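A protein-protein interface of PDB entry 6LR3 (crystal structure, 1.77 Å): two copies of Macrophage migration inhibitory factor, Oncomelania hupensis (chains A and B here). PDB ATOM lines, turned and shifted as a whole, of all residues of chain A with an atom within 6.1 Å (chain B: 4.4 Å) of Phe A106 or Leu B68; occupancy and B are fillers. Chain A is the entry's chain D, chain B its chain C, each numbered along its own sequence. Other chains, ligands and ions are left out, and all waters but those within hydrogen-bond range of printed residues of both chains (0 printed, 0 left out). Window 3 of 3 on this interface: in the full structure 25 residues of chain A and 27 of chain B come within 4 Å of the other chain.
The side-chain amide nitrogen (ND2) of Asn B73 lies within hydrogen-bond range of the backbone carbonyl oxygen (O) of Leu A105, 3.0 Å away. The backbone carbonyl oxygen of Ile B97 lies close to the side-chain sulfur of Cys A107 (3.6 Å). The backbone NH (N) of Ser A108 sits at hydrogen-bond distance from the backbone carbonyl oxygen (O) of Ile B97, at 2.8 Å. The backbone NH of Phe B99 sits at hydrogen-bond distance from the backbone carbonyl oxygen of Phe A106, 2.7 Å away.
N of Val B62 sits at hydrogen-bond distance from O of Arg B98, at 2.9 Å. O of Asn B69 lies close to OD1 of Asn B73, at 3.1 Å.
Val A102 touches Arg B98. O of Leu B68 touches CZ of Phe A106 (3.8 Å). Asn B73 touches Phe A106 (ND2 to CD2, 3.5 Å). Phe A106 touches Ile B97. Phe A106 touches Arg B98 (O to CA, 3.4 Å). Pro B101 touches Phe A106.
Of the printed residues of chain B, Val A102 touches Arg B98 (3.7 Å). Pro A103 touches none of the printed residues of chain B. Of chain B, only Leu B68, Asn B73, Ile B97, Arg B98, Phe B99 and Pro B101 come within 4 Å of Phe A106. Of the printed residues of chain A, Asn B73 touches Leu A105 (3.0 Å) and Phe A106 (3.5 Å). Of the printed residues of chain A, Ile B97 touches Phe A106, Cys A107 and Ser A108. Printed residues of chain A within 4 Å of Arg B98: Val A102 and Phe A106. Of the printed residues of chain A, Pro B101 touches Phe A106. The nearest printed residue of chain A that does not touch Phe B99 is Ser A108 (4.3 Å).
Of the 15 printed residues of chain B, 6 touch a printed residue of chain A. Printed residues of chain B that touch a printed residue of chain A: Leu B68, Asn B73, Ile B97, Arg B98, Phe B99 and Pro B101. Hydrophobic or aromatic side chains of chain A that line the printed part of chain B: Val A102 and Phe A106. Along chain A the printed residues that touch a printed residue of chain B span positions 102 to 108. Among the printed residues, 10 pairs touch across the chains. Among the printed residues, no Asp or Glu carboxylate lies within 4 Å of a Lys or Arg side-chain nitrogen of the other chain.
No position is printed for both chains. Of the 10 pairs that touch across the chains among the printed residues, none has its exchanged pair printed and touching as well.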
ATOM      1  N   VAL A 102      25.624  -0.519  34.252  1.00  0.00           N
ATOM      2  CA  VAL A 102      24.925  -0.002  33.054  1.00  0.00           C
ATOM      3  C   VAL A 102      25.155  -0.994  31.930  1.00  0.00           C
ATOM      4  O   VAL A 102      26.286  -1.334  31.638  1.00  0.00           O
ATOM      5  CB  VAL A 102      25.467   1.378  32.676  1.00  0.00           C
ATOM      6  CG1 VAL A 102      24.789   1.902  31.435  1.00  0.00           C
ATOM      7  CG2 VAL A 102      25.291   2.328  33.832  1.00  0.00           C
ATOM      8  N   PRO A 103      24.090  -1.486  31.281  1.00  0.00           N
ATOM      9  CA  PRO A 103      24.273  -2.358  30.120  1.00  0.00           C
ATOM     10  C   PRO A 103      24.879  -1.585  28.946  1.00  0.00           C
ATOM     11  O   PRO A 103      24.475  -0.476  28.654  1.00  0.00           O
ATOM     12  CB  PRO A 103      22.856  -2.822  29.770  1.00  0.00           C
ATOM     13  CG  PRO A 103      22.027  -2.475  31.001  1.00  0.00           C
ATOM     14  CD  PRO A 103      22.677  -1.242  31.593  1.00  0.00           C
ATOM     15  N   ALA A 104      25.830  -2.231  28.250  1.00  0.00           N
ATOM     16  CA  ALA A 104      26.528  -1.653  27.083  1.00  0.00           C
ATOM     17  C   ALA A 104      25.515  -1.158  26.039  1.00  0.00           C
ATOM     18  O   ALA A 104      25.759  -0.106  25.456  1.00  0.00           O
ATOM     19  CB  ALA A 104      27.444  -2.699  26.496  1.00  0.00           C
ATOM     20  N   LEU A 105      24.432  -1.901  25.795  1.00  0.00           N
ATOM     21  CA  LEU A 105      23.488  -1.557  24.718  1.00  0.00           C
ATOM     22  C   LEU A 105      22.407  -0.602  25.239  1.00  0.00           C
ATOM     23  O   LEU A 105      21.491  -0.285  24.479  1.00  0.00           O
ATOM     24  CB  LEU A 105      22.877  -2.821  24.122  1.00  0.00           C
ATOM     25  CG  LEU A 105      23.899  -3.749  23.464  1.00  0.00           C
ATOM     26  CD1 LEU A 105      23.184  -5.020  23.005  1.00  0.00           C
ATOM     27  CD2 LEU A 105      24.710  -3.023  22.373  1.00  0.00           C
ATOM     28  N   PHE A 106      22.544  -0.144  26.481  1.00  0.00           N
ATOM     29  CA  PHE A 106      21.629   0.851  27.086  1.00  0.00           C
ATOM     30  C   PHE A 106      22.394   2.138  27.376  1.00  0.00           C
ATOM     31  O   PHE A 106      21.913   2.997  28.151  1.00  0.00           O
ATOM     32  CB  PHE A 106      20.947   0.266  28.310  1.00  0.00           C
ATOM     33  CG  PHE A 106      19.789  -0.627  27.944  1.00  0.00           C
ATOM     34  CD1 PHE A 106      20.005  -1.821  27.282  1.00  0.00           C
ATOM     35  CD2 PHE A 106      18.490  -0.253  28.231  1.00  0.00           C
ATOM     36  CE1 PHE A 106      18.940  -2.647  26.951  1.00  0.00           C
ATOM     37  CE2 PHE A 106      17.421  -1.059  27.852  1.00  0.00           C
ATOM     38  CZ  PHE A 106      17.656  -2.246  27.192  1.00  0.00           C
ATOM     39  N   CYS A 107      23.486   2.358  26.670  1.00  0.00           N
ATOM     40  CA  CYS A 107      24.285   3.577  26.875  1.00  0.00           C
ATOM     41  C   CYS A 107      24.969   3.963  25.570  1.00  0.00           C
ATOM     42  O   CYS A 107      25.604   3.102  24.951  1.00  0.00           O
ATOM     43  CB  CYS A 107      25.255   3.348  28.006  1.00  0.00           C
ATOM     44  SG  CYS A 107      26.116   4.869  28.433  1.00  0.00           S
ATOM     45  N   SER A 108      24.782   5.187  25.129  1.00  0.00           N
ATOM     46  CA  SER A 108      25.399   5.699  23.885  1.00  0.00           C
ATOM     47  C   SER A 108      26.574   6.592  24.232  1.00  0.00           C
ATOM     48  O   SER A 108      26.572   7.268  25.288  1.00  0.00           O
ATOM     49  CB  SER A 108      24.421   6.423  23.025  1.00  0.00           C
ATOM     50  OG  SER A 108      23.920   7.558  23.717  1.00  0.00           O
ATOM     51  N   LEU A 113      26.152   2.858  20.413  1.00  0.00           N
ATOM     52  CA  LEU A 113      26.073   2.187  21.723  1.00  0.00           C
ATOM     53  C   LEU A 113      27.471   1.680  22.057  1.00  0.00           C
ATOM     54  O   LEU A 113      28.404   1.888  21.260  1.00  0.00           O
ATOM     55  CB  LEU A 113      25.048   1.057  21.659  1.00  0.00           C
ATOM     56  CG  LEU A 113      23.645   1.493  21.247  1.00  0.00           C
ATOM     57  CD1 LEU A 113      22.705   0.303  21.226  1.00  0.00           C
ATOM     58  CD2 LEU A 113      23.098   2.563  22.185  1.00  0.00           C
ATOM     59  N   LEU B  31       9.169   7.411  21.892  1.00  0.00           N
ATOM     60  CA  LEU B  31       8.824   6.392  22.914  1.00  0.00           C
ATOM     61  C   LEU B  31       7.363   5.956  22.778  1.00  0.00           C
ATOM     62  O   LEU B  31       6.998   4.999  23.441  1.00  0.00           O
ATOM     63  CB  LEU B  31       9.072   6.958  24.313  1.00  0.00           C
ATOM     64  CG  LEU B  31      10.562   7.183  24.607  1.00  0.00           C
ATOM     65  CD1 LEU B  31      10.761   7.948  25.908  1.00  0.00           C
ATOM     66  CD2 LEU B  31      11.318   5.879  24.694  1.00  0.00           C
ATOM     67  N   VAL B  62      17.332   8.517  29.997  1.00  0.00           N
ATOM     68  CA  VAL B  62      15.968   8.269  29.510  1.00  0.00           C
ATOM     69  C   VAL B  62      15.387   7.145  30.343  1.00  0.00           C
ATOM     70  O   VAL B  62      15.854   6.047  30.226  1.00  0.00           O
ATOM     71  CB  VAL B  62      15.963   7.917  28.019  1.00  0.00           C
ATOM     72  CG1 VAL B  62      14.556   7.610  27.544  1.00  0.00           C
ATOM     73  CG2 VAL B  62      16.616   9.033  27.197  1.00  0.00           C
ATOM     74  N   CYS B  64      12.114   4.990  31.151  1.00  0.00           N
ATOM     75  CA  CYS B  64      10.866   4.637  30.442  1.00  0.00           C
ATOM     76  C   CYS B  64      10.412   3.242  30.856  1.00  0.00           C
ATOM     77  O   CYS B  64      11.259   2.363  31.015  1.00  0.00           O
ATOM     78  CB  CYS B  64      11.068   4.712  28.938  1.00  0.00           C
ATOM     79  SG  CYS B  64       9.511   4.648  28.011  1.00  0.00           S
ATOM     80  N   GLY B  66       8.944   0.077  29.496  1.00  0.00           N
ATOM     81  CA  GLY B  66       9.000  -0.505  28.143  1.00  0.00           C
ATOM     82  C   GLY B  66       9.780   0.361  27.169  1.00  0.00           C
ATOM     83  O   GLY B  66      10.469   1.278  27.604  1.00  0.00           O
ATOM     84  N   ARG B  67       9.664   0.050  25.877  1.00  0.00           N
ATOM     85  CA  ARG B  67      10.128   0.867  24.728  1.00  0.00           C
ATOM     86  C   ARG B  67      11.639   0.835  24.533  1.00  0.00           C
ATOM     87  O   ARG B  67      12.057   1.131  23.415  1.00  0.00           O
ATOM     88  CB  ARG B  67       9.685   2.327  24.868  1.00  0.00           C
ATOM     89  CG  ARG B  67       8.194   2.488  25.081  1.00  0.00           C
ATOM     90  CD  ARG B  67       7.425   1.988  23.858  1.00  0.00           C
ATOM     91  NE  ARG B  67       6.095   2.545  23.982  1.00  0.00           N
ATOM     92  CZ  ARG B  67       5.087   1.977  24.626  1.00  0.00           C
ATOM     93  NH1 ARG B  67       5.221   0.784  25.180  1.00  0.00           N
ATOM     94  NH2 ARG B  67       3.937   2.619  24.736  1.00  0.00           N
ATOM     95  N   LEU B  68      12.439   0.545  25.554  1.00  0.00           N
ATOM     96  CA  LEU B  68      13.908   0.611  25.462  1.00  0.00           C
ATOM     97  C   LEU B  68      14.467  -0.755  25.068  1.00  0.00           C
ATOM     98  O   LEU B  68      14.208  -1.762  25.747  1.00  0.00           O
ATOM     99  CB  LEU B  68      14.474   1.075  26.795  1.00  0.00           C
ATOM    100  CG  LEU B  68      13.892   2.380  27.302  1.00  0.00           C
ATOM    101  CD1 LEU B  68      14.585   2.778  28.613  1.00  0.00           C
ATOM    102  CD2 LEU B  68      14.030   3.475  26.269  1.00  0.00           C
ATOM    103  N   ASN B  69      15.249  -0.747  24.000  1.00  0.00           N
ATOM    104  CA  ASN B  69      15.900  -1.952  23.459  1.00  0.00           C
ATOM    105  C   ASN B  69      17.044  -1.453  22.595  1.00  0.00           C
ATOM    106  O   ASN B  69      17.090  -0.276  22.268  1.00  0.00           O
ATOM    107  CB  ASN B  69      14.885  -2.820  22.717  1.00  0.00           C
ATOM    108  CG  ASN B  69      14.292  -2.108  21.520  1.00  0.00           C
ATOM    109  OD1 ASN B  69      14.981  -1.863  20.537  1.00  0.00           O
ATOM    110  ND2 ASN B  69      13.039  -1.726  21.600  1.00  0.00           N
ATOM    111  N   SER B  72      16.025   0.648  19.382  1.00  0.00           N
ATOM    112  CA  SER B  72      15.334   1.925  19.696  1.00  0.00           C
ATOM    113  C   SER B  72      16.331   2.831  20.408  1.00  0.00           C
ATOM    114  O   SER B  72      16.330   4.031  20.127  1.00  0.00           O
ATOM    115  CB  SER B  72      14.080   1.717  20.478  1.00  0.00           C
ATOM    116  OG  SER B  72      14.365   1.232  21.782  1.00  0.00           O
ATOM    117  N   ASN B  73      17.168   2.271  21.279  1.00  0.00           N
ATOM    118  CA  ASN B  73      18.155   3.070  22.058  1.00  0.00           C
ATOM    119  C   ASN B  73      19.085   3.787  21.079  1.00  0.00           C
ATOM    120  O   ASN B  73      19.354   4.993  21.257  1.00  0.00           O
ATOM    121  CB  ASN B  73      18.946   2.217  23.038  1.00  0.00           C
ATOM    122  CG  ASN B  73      18.107   1.648  24.175  1.00  0.00           C
ATOM    123  OD1 ASN B  73      16.942   2.041  24.389  1.00  0.00           O
ATOM    124  ND2 ASN B  73      18.698   0.712  24.920  1.00  0.00           N
ATOM    125  N   MET B  76      17.190   6.595  19.118  1.00  0.00           N
ATOM    126  CA  MET B  76      16.846   7.719  20.006  1.00  0.00           C
ATOM    127  C   MET B  76      18.131   8.431  20.384  1.00  0.00           C
ATOM    128  O   MET B  76      18.104   9.645  20.417  1.00  0.00           O
ATOM    129  CB  MET B  76      16.108   7.238  21.247  1.00  0.00           C
ATOM    130  CG  MET B  76      14.700   6.893  20.892  1.00  0.00           C
ATOM    131  SD  MET B  76      13.740   6.411  22.343  1.00  0.00           S
ATOM    132  CE  MET B  76      14.418   4.837  22.827  1.00  0.00           C
ATOM    133  N   ILE B  97      24.494   9.065  26.725  1.00  0.00           N
ATOM    134  CA  ILE B  97      23.063   8.899  27.097  1.00  0.00           C
ATOM    135  C   ILE B  97      22.874   7.496  27.661  1.00  0.00           C
ATOM    136  O   ILE B  97      23.284   6.536  27.031  1.00  0.00           O
ATOM    137  CB  ILE B  97      22.125   9.161  25.905  1.00  0.00           C
ATOM    138  CG1 ILE B  97      22.398  10.504  25.229  1.00  0.00           C
ATOM    139  CG2 ILE B  97      20.687   9.018  26.367  1.00  0.00           C
ATOM    140  CD1 ILE B  97      21.805  10.638  23.839  1.00  0.00           C
ATOM    141  N   ARG B  98      22.262   7.400  28.826  1.00  0.00           N
ATOM    142  CA  ARG B  98      21.918   6.113  29.444  1.00  0.00           C
ATOM    143  C   ARG B  98      20.408   5.932  29.343  1.00  0.00           C
ATOM    144  O   ARG B  98      19.638   6.819  29.708  1.00  0.00           O
ATOM    145  CB  ARG B  98      22.375   6.058  30.891  1.00  0.00           C
ATOM    146  CG  ARG B  98      21.996   4.781  31.606  1.00  0.00           C
ATOM    147  CD  ARG B  98      22.515   4.780  33.018  1.00  0.00           C
ATOM    148  NE  ARG B  98      21.826   3.709  33.696  1.00  0.00           N
ATOM    149  CZ  ARG B  98      21.406   3.719  34.938  1.00  0.00           C
ATOM    150  NH1 ARG B  98      21.692   4.718  35.752  1.00  0.00           N
ATOM    151  NH2 ARG B  98      20.673   2.703  35.372  1.00  0.00           N
ATOM    152  N   PHE B  99      20.017   4.757  28.869  1.00  0.00           N
ATOM    153  CA  PHE B  99      18.617   4.317  28.741  1.00  0.00           C
ATOM    154  C   PHE B  99      18.323   3.415  29.942  1.00  0.00           C
ATOM    155  O   PHE B  99      19.037   2.462  30.182  1.00  0.00           O
ATOM    156  CB  PHE B  99      18.426   3.663  27.380  1.00  0.00           C
ATOM    157  CG  PHE B  99      18.660   4.635  26.250  1.00  0.00           C
ATOM    158  CD1 PHE B  99      17.613   5.400  25.773  1.00  0.00           C
ATOM    159  CD2 PHE B  99      19.925   4.833  25.731  1.00  0.00           C
ATOM    160  CE1 PHE B  99      17.828   6.326  24.756  1.00  0.00           C
ATOM    161  CE2 PHE B  99      20.130   5.762  24.719  1.00  0.00           C
ATOM    162  CZ  PHE B  99      19.084   6.504  24.241  1.00  0.00           C
ATOM    163  N   ILE B 100      17.304   3.775  30.713  1.00  0.00           N
ATOM    164  CA  ILE B 100      16.979   3.157  32.023  1.00  0.00           C
ATOM    165  C   ILE B 100      15.576   2.566  31.962  1.00  0.00           C
ATOM    166  O   ILE B 100      14.574   3.277  32.038  1.00  0.00           O
ATOM    167  CB  ILE B 100      17.126   4.167  33.164  1.00  0.00           C
ATOM    168  CG1 ILE B 100      18.485   4.875  33.129  1.00  0.00           C
ATOM    169  CG2 ILE B 100      16.864   3.453  34.488  1.00  0.00           C
ATOM    170  CD1 ILE B 100      18.696   5.883  34.225  1.00  0.00           C
ATOM    171  N   PRO B 101      15.477   1.233  31.858  1.00  0.00           N
ATOM    172  CA  PRO B 101      14.185   0.549  31.858  1.00  0.00           C
ATOM    173  C   PRO B 101      13.582   0.612  33.255  1.00  0.00           C
ATOM    174  O   PRO B 101      14.305   0.453  34.232  1.00  0.00           O
ATOM    175  CB  PRO B 101      14.488  -0.906  31.479  1.00  0.00           C
ATOM    176  CG  PRO B 101      16.010  -1.044  31.433  1.00  0.00           C
ATOM    177  CD  PRO B 101      16.619   0.311  31.691  1.00  0.00           C
